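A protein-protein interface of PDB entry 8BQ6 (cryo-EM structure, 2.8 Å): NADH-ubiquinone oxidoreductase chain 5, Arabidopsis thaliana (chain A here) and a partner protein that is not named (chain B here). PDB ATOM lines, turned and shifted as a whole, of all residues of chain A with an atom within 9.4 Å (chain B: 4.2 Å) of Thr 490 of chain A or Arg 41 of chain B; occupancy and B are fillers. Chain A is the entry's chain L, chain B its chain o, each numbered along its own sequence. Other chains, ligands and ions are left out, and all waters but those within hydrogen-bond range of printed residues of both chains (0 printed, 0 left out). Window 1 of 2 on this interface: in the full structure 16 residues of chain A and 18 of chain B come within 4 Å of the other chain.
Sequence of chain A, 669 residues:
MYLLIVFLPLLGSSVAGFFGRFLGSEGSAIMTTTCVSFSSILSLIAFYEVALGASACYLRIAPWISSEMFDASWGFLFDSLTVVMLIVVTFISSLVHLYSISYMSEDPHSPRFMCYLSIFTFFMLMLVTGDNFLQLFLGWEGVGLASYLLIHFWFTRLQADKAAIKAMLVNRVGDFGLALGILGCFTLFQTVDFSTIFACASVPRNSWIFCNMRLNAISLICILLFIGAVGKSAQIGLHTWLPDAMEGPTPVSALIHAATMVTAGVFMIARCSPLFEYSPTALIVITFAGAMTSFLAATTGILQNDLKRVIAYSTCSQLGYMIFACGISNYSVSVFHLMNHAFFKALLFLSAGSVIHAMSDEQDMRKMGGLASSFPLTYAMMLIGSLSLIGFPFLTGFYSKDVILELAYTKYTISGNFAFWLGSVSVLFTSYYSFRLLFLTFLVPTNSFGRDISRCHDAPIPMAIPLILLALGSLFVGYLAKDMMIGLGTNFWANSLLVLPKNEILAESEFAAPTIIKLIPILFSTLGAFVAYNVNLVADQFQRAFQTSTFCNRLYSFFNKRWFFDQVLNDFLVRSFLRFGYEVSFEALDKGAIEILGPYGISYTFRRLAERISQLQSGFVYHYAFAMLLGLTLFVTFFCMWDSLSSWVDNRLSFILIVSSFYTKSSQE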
ATOM      1  N   ALA A  51     -21.348  -9.760  16.082  1.00  0.00           N
ATOM      2  CA  ALA A  51     -21.973 -10.604  17.094  1.00  0.00           C
ATOM      3  C   ALA A  51     -22.620  -9.769  18.192  1.00  0.00           C
ATOM      4  O   ALA A  51     -23.785  -9.979  18.545  1.00  0.00           O
ATOM      5  CB  ALA A  51     -20.939 -11.561  17.687  1.00  0.00           C
ATOM      6  N   LEU A  52     -21.867  -8.822  18.755  1.00  0.00           N
ATOM      7  CA  LEU A  52     -22.404  -7.995  19.828  1.00  0.00           C
ATOM      8  C   LEU A  52     -23.384  -6.960  19.293  1.00  0.00           C
ATOM      9  O   LEU A  52     -24.393  -6.659  19.941  1.00  0.00           O
ATOM     10  CB  LEU A  52     -21.263  -7.319  20.585  1.00  0.00           C
ATOM     11  CG  LEU A  52     -20.214  -8.283  21.134  1.00  0.00           C
ATOM     12  CD1 LEU A  52     -19.150  -7.536  21.914  1.00  0.00           C
ATOM     13  CD2 LEU A  52     -20.880  -9.334  22.001  1.00  0.00           C
ATOM     14  N   GLY A  53     -23.105  -6.410  18.109  1.00  0.00           N
ATOM     15  CA  GLY A  53     -23.978  -5.379  17.516  1.00  0.00           C
ATOM     16  C   GLY A  53     -25.079  -5.968  16.657  1.00  0.00           C
ATOM     17  O   GLY A  53     -25.879  -5.181  16.147  1.00  0.00           O
ATOM     18  N   SER A  80     -22.386 -14.517  13.010  1.00  0.00           N
ATOM     19  CA  SER A  80     -21.954 -14.777  14.378  1.00  0.00           C
ATOM     20  C   SER A  80     -21.000 -15.962  14.450  1.00  0.00           C
ATOM     21  O   SER A  80     -20.014 -15.934  15.196  1.00  0.00           O
ATOM     22  CB  SER A  80     -23.175 -15.005  15.264  1.00  0.00           C
ATOM     23  OG  SER A  80     -23.783 -13.768  15.574  1.00  0.00           O
ATOM     24  N   SER A 332     -24.360 -25.086  18.945  1.00  0.00           N
ATOM     25  CA  SER A 332     -23.834 -24.021  19.788  1.00  0.00           C
ATOM     26  C   SER A 332     -22.916 -24.579  20.864  1.00  0.00           C
ATOM     27  O   SER A 332     -21.945 -23.928  21.260  1.00  0.00           O
ATOM     28  CB  SER A 332     -24.981 -23.234  20.416  1.00  0.00           C
ATOM     29  OG  SER A 332     -25.783 -24.074  21.226  1.00  0.00           O
ATOM     30  N   VAL A 333     -23.212 -25.783  21.352  1.00  0.00           N
ATOM     31  CA  VAL A 333     -22.359 -26.398  22.360  1.00  0.00           C
ATOM     32  C   VAL A 333     -21.046 -26.867  21.747  1.00  0.00           C
ATOM     33  O   VAL A 333     -19.978 -26.718  22.351  1.00  0.00           O
ATOM     34  CB  VAL A 333     -23.101 -27.550  23.057  1.00  0.00           C
ATOM     35  CG1 VAL A 333     -22.362 -27.958  24.313  1.00  0.00           C
ATOM     36  CG2 VAL A 333     -24.519 -27.131  23.381  1.00  0.00           C
ATOM     37  N   ALA A 481     -18.121 -16.664  28.572  1.00  0.00           N
ATOM     38  CA  ALA A 481     -18.768 -16.810  27.277  1.00  0.00           C
ATOM     39  C   ALA A 481     -19.915 -17.811  27.273  1.00  0.00           C
ATOM     40  O   ALA A 481     -20.487 -18.061  26.207  1.00  0.00           O
ATOM     41  CB  ALA A 481     -17.734 -17.208  26.216  1.00  0.00           C
ATOM     42  N   LYS A 482     -20.278 -18.380  28.425  1.00  0.00           N
ATOM     43  CA  LYS A 482     -21.343 -19.381  28.451  1.00  0.00           C
ATOM     44  C   LYS A 482     -22.689 -18.780  28.068  1.00  0.00           C
ATOM     45  O   LYS A 482     -23.317 -19.209  27.094  1.00  0.00           O
ATOM     46  CB  LYS A 482     -21.450 -20.026  29.828  1.00  0.00           C
ATOM     47  CG  LYS A 482     -22.683 -20.905  29.931  1.00  0.00           C
ATOM     48  CD  LYS A 482     -22.658 -21.803  31.140  1.00  0.00           C
ATOM     49  CE  LYS A 482     -24.068 -22.021  31.659  1.00  0.00           C
ATOM     50  NZ  LYS A 482     -24.984 -22.459  30.566  1.00  0.00           N
ATOM     51  N   ASP A 483     -23.164 -17.802  28.845  1.00  0.00           N
ATOM     52  CA  ASP A 483     -24.482 -17.232  28.584  1.00  0.00           C
ATOM     53  C   ASP A 483     -24.543 -16.636  27.185  1.00  0.00           C
ATOM     54  O   ASP A 483     -25.580 -16.695  26.515  1.00  0.00           O
ATOM     55  CB  ASP A 483     -24.827 -16.184  29.643  1.00  0.00           C
ATOM     56  CG  ASP A 483     -26.288 -15.769  29.597  1.00  0.00           C
ATOM     57  OD1 ASP A 483     -27.157 -16.622  29.871  1.00  0.00           O
ATOM     58  OD2 ASP A 483     -26.568 -14.589  29.306  1.00  0.00           O
ATOM     59  N   MET A 484     -23.430 -16.069  26.721  1.00  0.00           N
ATOM     60  CA  MET A 484     -23.352 -15.644  25.331  1.00  0.00           C
ATOM     61  C   MET A 484     -23.594 -16.809  24.379  1.00  0.00           C
ATOM     62  O   MET A 484     -24.450 -16.726  23.494  1.00  0.00           O
ATOM     63  CB  MET A 484     -21.993 -15.011  25.053  1.00  0.00           C
ATOM     64  CG  MET A 484     -22.039 -13.868  24.073  1.00  0.00           C
ATOM     65  SD  MET A 484     -20.394 -13.409  23.522  1.00  0.00           S
ATOM     66  CE  MET A 484     -19.696 -15.029  23.214  1.00  0.00           C
ATOM     67  N   MET A 485     -22.872 -17.913  24.558  1.00  0.00           N
ATOM     68  CA  MET A 485     -22.898 -18.986  23.572  1.00  0.00           C
ATOM     69  C   MET A 485     -24.041 -19.969  23.763  1.00  0.00           C
ATOM     70  O   MET A 485     -24.833 -20.168  22.837  1.00  0.00           O
ATOM     71  CB  MET A 485     -21.576 -19.761  23.578  1.00  0.00           C
ATOM     72  CG  MET A 485     -20.350 -18.934  23.211  1.00  0.00           C
ATOM     73  SD  MET A 485     -20.189 -18.653  21.441  1.00  0.00           S
ATOM     74  CE  MET A 485     -18.739 -19.615  21.018  1.00  0.00           C
ATOM     75  N   ILE A 486     -24.144 -20.603  24.932  1.00  0.00           N
ATOM     76  CA  ILE A 486     -25.163 -21.614  25.173  1.00  0.00           C
ATOM     77  C   ILE A 486     -26.117 -21.229  26.290  1.00  0.00           C
ATOM     78  O   ILE A 486     -26.706 -22.112  26.916  1.00  0.00           O
ATOM     79  CB  ILE A 486     -24.527 -22.986  25.463  1.00  0.00           C
ATOM     80  CG1 ILE A 486     -23.641 -22.899  26.706  1.00  0.00           C
ATOM     81  CG2 ILE A 486     -23.715 -23.445  24.265  1.00  0.00           C
ATOM     82  CD1 ILE A 486     -23.122 -24.226  27.170  1.00  0.00           C
ATOM     83  N   GLY A 487     -26.277 -19.939  26.574  1.00  0.00           N
ATOM     84  CA  GLY A 487     -27.303 -19.484  27.486  1.00  0.00           C
ATOM     85  C   GLY A 487     -28.670 -19.891  26.986  1.00  0.00           C
ATOM     86  O   GLY A 487     -28.940 -19.826  25.783  1.00  0.00           O
ATOM     87  N   LEU A 488     -29.535 -20.326  27.892  1.00  0.00           N
ATOM     88  CA  LEU A 488     -30.832 -20.855  27.494  1.00  0.00           C
ATOM     89  C   LEU A 488     -31.648 -19.779  26.788  1.00  0.00           C
ATOM     90  O   LEU A 488     -31.900 -18.707  27.345  1.00  0.00           O
ATOM     91  CB  LEU A 488     -31.562 -21.385  28.730  1.00  0.00           C
ATOM     92  CG  LEU A 488     -32.690 -22.395  28.520  1.00  0.00           C
ATOM     93  CD1 LEU A 488     -32.863 -23.301  29.735  1.00  0.00           C
ATOM     94  CD2 LEU A 488     -33.979 -21.680  28.221  1.00  0.00           C
ATOM     95  N   GLY A 489     -32.036 -20.063  25.545  1.00  0.00           N
ATOM     96  CA  GLY A 489     -32.771 -19.115  24.735  1.00  0.00           C
ATOM     97  C   GLY A 489     -31.958 -17.983  24.146  1.00  0.00           C
ATOM     98  O   GLY A 489     -32.549 -16.997  23.693  1.00  0.00           O
ATOM     99  N   THR A 490     -30.630 -18.092  24.122  1.00  0.00           N
ATOM    100  CA  THR A 490     -29.801 -16.984  23.659  1.00  0.00           C
ATOM    101  C   THR A 490     -30.038 -16.704  22.180  1.00  0.00           C
ATOM    102  O   THR A 490     -30.339 -17.610  21.397  1.00  0.00           O
ATOM    103  CB  THR A 490     -28.317 -17.278  23.905  1.00  0.00           C
ATOM    104  OG1 THR A 490     -27.533 -16.142  23.519  1.00  0.00           O
ATOM    105  CG2 THR A 490     -27.855 -18.493  23.107  1.00  0.00           C
ATOM    106  N   ASN A 491     -29.923 -15.428  21.805  1.00  0.00           N
ATOM    107  CA  ASN A 491     -30.030 -14.989  20.420  1.00  0.00           C
ATOM    108  C   ASN A 491     -28.684 -14.582  19.835  1.00  0.00           C
ATOM    109  O   ASN A 491     -28.640 -13.871  18.825  1.00  0.00           O
ATOM    110  CB  ASN A 491     -31.005 -13.820  20.302  1.00  0.00           C
ATOM    111  CG  ASN A 491     -30.561 -12.613  21.098  1.00  0.00           C
ATOM    112  OD1 ASN A 491     -29.648 -12.692  21.921  1.00  0.00           O
ATOM    113  ND2 ASN A 491     -31.179 -11.474  20.825  1.00  0.00           N
ATOM    114  N   PHE A 492     -27.589 -14.999  20.467  1.00  0.00           N
ATOM    115  CA  PHE A 492     -26.258 -14.582  20.039  1.00  0.00           C
ATOM    116  C   PHE A 492     -25.949 -15.061  18.629  1.00  0.00           C
ATOM    117  O   PHE A 492     -25.328 -14.343  17.838  1.00  0.00           O
ATOM    118  CB  PHE A 492     -25.235 -15.112  21.039  1.00  0.00           C
ATOM    119  CG  PHE A 492     -23.812 -14.991  20.594  1.00  0.00           C
ATOM    120  CD1 PHE A 492     -23.173 -13.769  20.591  1.00  0.00           C
ATOM    121  CD2 PHE A 492     -23.103 -16.116  20.213  1.00  0.00           C
ATOM    122  CE1 PHE A 492     -21.859 -13.669  20.201  1.00  0.00           C
ATOM    123  CE2 PHE A 492     -21.790 -16.019  19.818  1.00  0.00           C
ATOM    124  CZ  PHE A 492     -21.166 -14.796  19.812  1.00  0.00           C
ATOM    125  N   TRP A 493     -26.385 -16.273  18.294  1.00  0.00           N
ATOM    126  CA  TRP A 493     -26.090 -16.857  16.996  1.00  0.00           C
ATOM    127  C   TRP A 493     -26.995 -16.339  15.891  1.00  0.00           C
ATOM    128  O   TRP A 493     -26.695 -16.567  14.716  1.00  0.00           O
ATOM    129  CB  TRP A 493     -26.208 -18.374  17.079  1.00  0.00           C
ATOM    130  CG  TRP A 493     -25.289 -18.959  18.081  1.00  0.00           C
ATOM    131  CD1 TRP A 493     -25.608 -19.389  19.331  1.00  0.00           C
ATOM    132  CD2 TRP A 493     -23.886 -19.173  17.925  1.00  0.00           C
ATOM    133  NE1 TRP A 493     -24.489 -19.866  19.965  1.00  0.00           N
ATOM    134  CE2 TRP A 493     -23.419 -19.744  19.119  1.00  0.00           C
ATOM    135  CE3 TRP A 493     -22.981 -18.942  16.887  1.00  0.00           C
ATOM    136  CZ2 TRP A 493     -22.089 -20.091  19.303  1.00  0.00           C
ATOM    137  CZ3 TRP A 493     -21.662 -19.279  17.075  1.00  0.00           C
ATOM    138  CH2 TRP A 493     -21.226 -19.844  18.275  1.00  0.00           C
ATOM    139  N   ALA A 494     -28.086 -15.656  16.243  1.00  0.00           N
ATOM    140  CA  ALA A 494     -29.032 -15.133  15.264  1.00  0.00           C
ATOM    141  C   ALA A 494     -29.503 -16.243  14.335  1.00  0.00           C
ATOM    142  O   ALA A 494     -30.198 -17.167  14.767  1.00  0.00           O
ATOM    143  CB  ALA A 494     -28.408 -13.986  14.466  1.00  0.00           C
ATOM    144  N   ASN A 495     -29.119 -16.172  13.062  1.00  0.00           N
ATOM    145  CA  ASN A 495     -29.463 -17.197  12.088  1.00  0.00           C
ATOM    146  C   ASN A 495     -28.265 -18.042  11.675  1.00  0.00           C
ATOM    147  O   ASN A 495     -28.329 -18.732  10.652  1.00  0.00           O
ATOM    148  CB  ASN A 495     -30.099 -16.560  10.853  1.00  0.00           C
ATOM    149  CG  ASN A 495     -31.079 -17.485  10.165  1.00  0.00           C
ATOM    150  OD1 ASN A 495     -31.552 -18.453  10.756  1.00  0.00           O
ATOM    151  ND2 ASN A 495     -31.372 -17.203   8.904  1.00  0.00           N
ATOM    152  N   LEU A 497     -26.778 -20.646  13.345  1.00  0.00           N
ATOM    153  CA  LEU A 497     -27.019 -22.050  13.624  1.00  0.00           C
ATOM    154  C   LEU A 497     -28.513 -22.309  13.668  1.00  0.00           C
ATOM    155  O   LEU A 497     -29.307 -21.423  13.998  1.00  0.00           O
ATOM    156  CB  LEU A 497     -26.369 -22.480  14.942  1.00  0.00           C
ATOM    157  CG  LEU A 497     -24.872 -22.192  14.989  1.00  0.00           C
ATOM    158  CD1 LEU A 497     -24.333 -22.253  16.405  1.00  0.00           C
ATOM    159  CD2 LEU A 497     -24.137 -23.162  14.082  1.00  0.00           C
ATOM    160  N   VAL A 499     -31.371 -25.168  15.052  1.00  0.00           N
ATOM    161  CA  VAL A 499     -31.843 -26.351  15.759  1.00  0.00           C
ATOM    162  C   VAL A 499     -33.358 -26.371  15.620  1.00  0.00           C
ATOM    163  O   VAL A 499     -34.035 -25.428  16.045  1.00  0.00           O
ATOM    164  CB  VAL A 499     -31.422 -26.347  17.236  1.00  0.00           C
ATOM    165  CG1 VAL A 499     -31.706 -27.698  17.872  1.00  0.00           C
ATOM    166  CG2 VAL A 499     -29.950 -25.990  17.371  1.00  0.00           C
ATOM    167  N   GLU A 504     -34.758 -29.903  20.251  1.00  0.00           N
ATOM    168  CA  GLU A 504     -34.242 -29.077  21.335  1.00  0.00           C
ATOM    169  C   GLU A 504     -34.298 -29.838  22.654  1.00  0.00           C
ATOM    170  O   GLU A 504     -35.354 -30.344  23.046  1.00  0.00           O
ATOM    171  CB  GLU A 504     -35.027 -27.773  21.423  1.00  0.00           C
ATOM    172  CG  GLU A 504     -35.088 -27.033  20.106  1.00  0.00           C
ATOM    173  CD  GLU A 504     -33.947 -26.047  19.945  1.00  0.00           C
ATOM    174  OE1 GLU A 504     -32.987 -26.110  20.740  1.00  0.00           O
ATOM    175  OE2 GLU A 504     -34.000 -25.222  19.012  1.00  0.00           O
ATOM    176  N   LEU A 506     -31.883 -28.713  25.439  1.00  0.00           N
ATOM    177  CA  LEU A 506     -31.035 -28.036  26.421  1.00  0.00           C
ATOM    178  C   LEU A 506     -31.751 -27.867  27.756  1.00  0.00           C
ATOM    179  O   LEU A 506     -31.163 -28.102  28.818  1.00  0.00           O
ATOM    180  CB  LEU A 506     -30.568 -26.679  25.892  1.00  0.00           C
ATOM    181  CG  LEU A 506     -29.636 -25.937  26.863  1.00  0.00           C
ATOM    182  CD1 LEU A 506     -28.259 -26.586  26.934  1.00  0.00           C
ATOM    183  CD2 LEU A 506     -29.513 -24.458  26.520  1.00  0.00           C
ATOM    184  N   LEU B  34     -38.628 -14.378  27.515  1.00  0.00           N
ATOM    185  CA  LEU B  34     -37.360 -14.385  26.793  1.00  0.00           C
ATOM    186  C   LEU B  34     -37.086 -13.031  26.152  1.00  0.00           C
ATOM    187  O   LEU B  34     -35.943 -12.561  26.140  1.00  0.00           O
ATOM    188  CB  LEU B  34     -37.367 -15.493  25.740  1.00  0.00           C
ATOM    189  CG  LEU B  34     -36.190 -15.584  24.768  1.00  0.00           C
ATOM    190  CD1 LEU B  34     -34.867 -15.629  25.512  1.00  0.00           C
ATOM    191  CD2 LEU B  34     -36.346 -16.812  23.896  1.00  0.00           C
ATOM    192  N   LEU B  37     -35.390 -10.756  28.400  1.00  0.00           N
ATOM    193  CA  LEU B  37     -34.073 -11.308  28.695  1.00  0.00           C
ATOM    194  C   LEU B  37     -33.078 -11.021  27.576  1.00  0.00           C
ATOM    195  O   LEU B  37     -31.962 -10.556  27.836  1.00  0.00           O
ATOM    196  CB  LEU B  37     -34.197 -12.809  28.939  1.00  0.00           C
ATOM    197  CG  LEU B  37     -32.929 -13.562  29.308  1.00  0.00           C
ATOM    198  CD1 LEU B  37     -32.189 -12.815  30.390  1.00  0.00           C
ATOM    199  CD2 LEU B  37     -33.328 -14.930  29.797  1.00  0.00           C
ATOM    200  N   ASN B  38     -33.463 -11.283  26.324  1.00  0.00           N
ATOM    201  CA  ASN B  38     -32.538 -11.083  25.211  1.00  0.00           C
ATOM    202  C   ASN B  38     -32.248  -9.610  24.965  1.00  0.00           C
ATOM    203  O   ASN B  38     -31.166  -9.267  24.474  1.00  0.00           O
ATOM    204  CB  ASN B  38     -33.092 -11.711  23.937  1.00  0.00           C
ATOM    205  CG  ASN B  38     -32.898 -13.208  23.895  1.00  0.00           C
ATOM    206  OD1 ASN B  38     -32.202 -13.782  24.731  1.00  0.00           O
ATOM    207  ND2 ASN B  38     -33.514 -13.850  22.913  1.00  0.00           N
ATOM    208  N   LYS B  39     -33.206  -8.732  25.259  1.00  0.00           N
ATOM    209  CA  LYS B  39     -32.948  -7.303  25.138  1.00  0.00           C
ATOM    210  C   LYS B  39     -31.990  -6.836  26.222  1.00  0.00           C
ATOM    211  O   LYS B  39     -31.169  -5.940  26.001  1.00  0.00           O
ATOM    212  CB  LYS B  39     -34.260  -6.526  25.199  1.00  0.00           C
ATOM    213  CG  LYS B  39     -35.101  -6.672  23.952  1.00  0.00           C
ATOM    214  CD  LYS B  39     -35.289  -5.338  23.265  1.00  0.00           C
ATOM    215  CE  LYS B  39     -36.699  -4.818  23.480  1.00  0.00           C
ATOM    216  NZ  LYS B  39     -36.927  -3.524  22.787  1.00  0.00           N
ATOM    217  N   CYS B  40     -32.086  -7.429  27.411  1.00  0.00           N
ATOM    218  CA  CYS B  40     -31.090  -7.152  28.436  1.00  0.00           C
ATOM    219  C   CYS B  40     -29.740  -7.738  28.050  1.00  0.00           C
ATOM    220  O   CYS B  40     -28.697  -7.124  28.294  1.00  0.00           O
ATOM    221  CB  CYS B  40     -31.549  -7.703  29.785  1.00  0.00           C
ATOM    222  SG  CYS B  40     -30.508  -7.210  31.179  1.00  0.00           S
ATOM    223  N   ARG B  41     -29.741  -8.925  27.443  1.00  0.00           N
ATOM    224  CA  ARG B  41     -28.485  -9.588  27.122  1.00  0.00           C
ATOM    225  C   ARG B  41     -27.696  -8.813  26.075  1.00  0.00           C
ATOM    226  O   ARG B  41     -26.482  -8.622  26.216  1.00  0.00           O
ATOM    227  CB  ARG B  41     -28.761 -11.016  26.659  1.00  0.00           C
ATOM    228  CG  ARG B  41     -28.806 -12.005  27.804  1.00  0.00           C
ATOM    229  CD  ARG B  41     -28.648 -13.421  27.318  1.00  0.00           C
ATOM    230  NE  ARG B  41     -29.911 -14.041  26.945  1.00  0.00           N
ATOM    231  CZ  ARG B  41     -30.280 -15.253  27.337  1.00  0.00           C
ATOM    232  NH1 ARG B  41     -29.517 -15.981  28.136  1.00  0.00           N
ATOM    233  NH2 ARG B  41     -31.441 -15.746  26.916  1.00  0.00           N
ATOM    234  N   GLN B  42     -28.367  -8.346  25.020  1.00  0.00           N
ATOM    235  CA  GLN B  42     -27.675  -7.572  23.995  1.00  0.00           C
ATOM    236  C   GLN B  42     -27.167  -6.251  24.548  1.00  0.00           C
ATOM    237  O   GLN B  42     -26.028  -5.852  24.279  1.00  0.00           O
ATOM    238  CB  GLN B  42     -28.606  -7.325  22.815  1.00  0.00           C
ATOM    239  CG  GLN B  42     -28.645  -8.468  21.846  1.00  0.00           C
ATOM    240  CD  GLN B  42     -29.414  -8.129  20.599  1.00  0.00           C
ATOM    241  OE1 GLN B  42     -30.416  -7.414  20.650  1.00  0.00           O
ATOM    242  NE2 GLN B  42     -28.965  -8.655  19.467  1.00  0.00           N
ATOM    243  N   ALA B  43     -28.001  -5.559  25.326  1.00  0.00           N
ATOM    244  CA  ALA B  43     -27.611  -4.267  25.873  1.00  0.00           C
ATOM    245  C   ALA B  43     -26.457  -4.388  26.859  1.00  0.00           C
ATOM    246  O   ALA B  43     -25.709  -3.424  27.053  1.00  0.00           O
ATOM    247  CB  ALA B  43     -28.816  -3.603  26.537  1.00  0.00           C
ATOM    248  N   GLU B  44     -26.285  -5.552  27.483  1.00  0.00           N
ATOM    249  CA  GLU B  44     -25.242  -5.739  28.481  1.00  0.00           C
ATOM    250  C   GLU B  44     -24.089  -6.595  27.978  1.00  0.00           C
ATOM    251  O   GLU B  44     -23.356  -7.147  28.796  1.00  0.00           O
ATOM    252  CB  GLU B  44     -25.826  -6.346  29.759  1.00  0.00           C
ATOM    253  CG  GLU B  44     -27.010  -5.582  30.336  1.00  0.00           C
ATOM    254  CD  GLU B  44     -26.680  -4.138  30.651  1.00  0.00           C
ATOM    255  OE1 GLU B  44     -25.961  -3.895  31.643  1.00  0.00           O
ATOM    256  OE2 GLU B  44     -27.147  -3.244  29.913  1.00  0.00           O
ATOM    257  N   PHE B  45     -23.924  -6.727  26.659  1.00  0.00           N
ATOM    258  CA  PHE B  45     -22.817  -7.475  26.052  1.00  0.00           C
ATOM    259  C   PHE B  45     -22.740  -8.914  26.555  1.00  0.00           C
ATOM    260  O   PHE B  45     -21.668  -9.523  26.551  1.00  0.00           O
ATOM    261  CB  PHE B  45     -21.477  -6.773  26.276  1.00  0.00           C
ATOM    262  CG  PHE B  45     -21.441  -5.384  25.756  1.00  0.00           C
ATOM    263  CD1 PHE B  45     -21.058  -5.138  24.455  1.00  0.00           C
ATOM    264  CD2 PHE B  45     -21.803  -4.321  26.561  1.00  0.00           C
ATOM    265  CE1 PHE B  45     -21.027  -3.864  23.964  1.00  0.00           C
ATOM    266  CE2 PHE B  45     -21.777  -3.039  26.073  1.00  0.00           C
ATOM    267  CZ  PHE B  45     -21.388  -2.809  24.770  1.00  0.00           C
ATOM    268  N   TYR B  46     -23.874  -9.455  27.000  1.00  0.00           N
ATOM    269  CA  TYR B  46     -23.990 -10.851  27.423  1.00  0.00           C
ATOM    270  C   TYR B  46     -23.044 -11.219  28.563  1.00  0.00           C
ATOM    271  O   TYR B  46     -22.580 -12.358  28.632  1.00  0.00           O
ATOM    272  CB  TYR B  46     -23.745 -11.824  26.268  1.00  0.00           C
ATOM    273  CG  TYR B  46     -24.664 -11.697  25.085  1.00  0.00           C
ATOM    274  CD1 TYR B  46     -24.370 -10.830  24.047  1.00  0.00           C
ATOM    275  CD2 TYR B  46     -25.820 -12.455  25.001  1.00  0.00           C
ATOM    276  CE1 TYR B  46     -25.204 -10.717  22.960  1.00  0.00           C
ATOM    277  CE2 TYR B  46     -26.660 -12.348  23.919  1.00  0.00           C
ATOM    278  CZ  TYR B  46     -26.346 -11.479  22.901  1.00  0.00           C
ATOM    279  OH  TYR B  46     -27.179 -11.364  21.816  1.00  0.00           O
ATOM    280  N   CYS B  51     -28.200  -9.032  34.091  1.00  0.00           N
ATOM    281  CA  CYS B  51     -29.519  -9.562  33.754  1.00  0.00           C
ATOM    282  C   CYS B  51     -29.876 -10.793  34.571  1.00  0.00           C
ATOM    283  O   CYS B  51     -30.688 -11.612  34.132  1.00  0.00           O
ATOM    284  CB  CYS B  51     -29.627  -9.887  32.262  1.00  0.00           C
ATOM    285  SG  CYS B  51     -29.011  -8.582  31.200  1.00  0.00           S
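OG of Ser 80 of chain A is in hydrogen-bond range of O of Phe 492 of chain A (2.8 Å).
The backbone carbonyl oxygen (O) of Met 484 of chain A lies within hydrogen-bond range of the side-chain hydroxyl (OG1) of Thr 490 of chain A, at 3.1 Å.
The backbone NH (N) of Phe 492 of chain A sits at hydrogen-bond distance from the side-chain hydroxyl (OG1) of Thr 490 of chain A, at 3.3 Å.
The side-chain amide oxygen (OD1) of Asn 38 of chain B lies within hydrogen-bond range of the guanidinium group (NH2) of Arg 41 of chain B.
The backbone carbonyl oxygen (O) of Arg 41 of chain B is in hydrogen-bond range of the backbone NH (N) of Tyr 46 of chain B (2.8 Å).
The side-chain sulfur (SG) of Cys 40 of chain B is disulfide-bonded to the side-chain sulfur (SG) of Cys 51 of chain B (2.0 Å).
Leu 52 of chain A touches Phe 45 of chain B.
CB of Tyr 46 of chain B touches CG of Met 484 of chain A, 3.5 Å away.
Leu 34 of chain B touches Gly 489 of chain A.
Gly 489 of chain A touches Arg 41 of chain B.
Thr 490 of chain A touches Arg 41 of chain B (N to NH2, 3.7 Å).
Thr 490 of chain A touches Tyr 46 of chain B (OG1 to CE2, 3.9 Å).
Asn 38 of chain B touches Asn 491 of chain A (ND2 to CB, 3.6 Å).
Gln 42 of chain B touches Asn 491 of chain A.
CA of Phe 492 of chain A touches OH of Tyr 46 of chain B (3.8 Å).
Of the printed residues of chain B, Asp 483 of chain A touches Arg 41.
Of the printed residues of chain B, Met 484 of chain A touches Tyr 46 (3.5 Å).
Thr 490 of chain A touches just these residues of chain B: Arg 41 (3.7 Å) and Tyr 46 (3.9 Å).
Leu 37 of chain B touches none of the printed residues of chain A.
Arg 41 of chain B touches just these residues of chain A: Asp 483 (3.0 Å), Leu 488 (3.0 Å), Gly 489 (3.6 Å) and Thr 490 (3.7 Å).
Ala 43 of chain B touches none of the printed residues of chain A.
The nearest residue of chain B that does not touch Thr 490 of chain A is Asn 38 of chain B (4.1 Å).
The nearest printed residue of chain B that does not touch Leu 488 of chain A is Leu 34 of chain B (4.7 Å).
Hydrophobic or aromatic side chains of chain B within 4 Å of the printed part of chain A: Leu 34, Phe 45 and Tyr 46.
Printed residues of chain A that touch a printed residue of chain B: Leu 52, Asp 483, Met 484, Leu 488, Gly 489, Thr 490, Asn 491 and Phe 492.
Among the printed residues, Asp or Glu carboxylates within 4 Å of a Lys or Arg side-chain nitrogen of the other chain: Asp 483 of chain A with Arg 41 of chain B (3.0 Å).
The side-chain carboxylate (OD1) of Asp 483 of chain A is in salt-bridge range of the guanidinium group (NH1) of Arg 41 of chain B (3.0 Å).
The guanidinium group (NH2) of Arg 41 of chain B sits at hydrogen-bond distance from the backbone carbonyl oxygen (O) of Leu 488 of chain A (3.0 Å).
The backbone carbonyl oxygen of Gly 489 of chain A is in hydrogen-bond range of the side-chain amide nitrogen of Asn 38 of chain B.
OH of Tyr 46 of chain B lies within hydrogen-bond range of OD1 of Asn 491 of chain A, at 2.8 Å.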
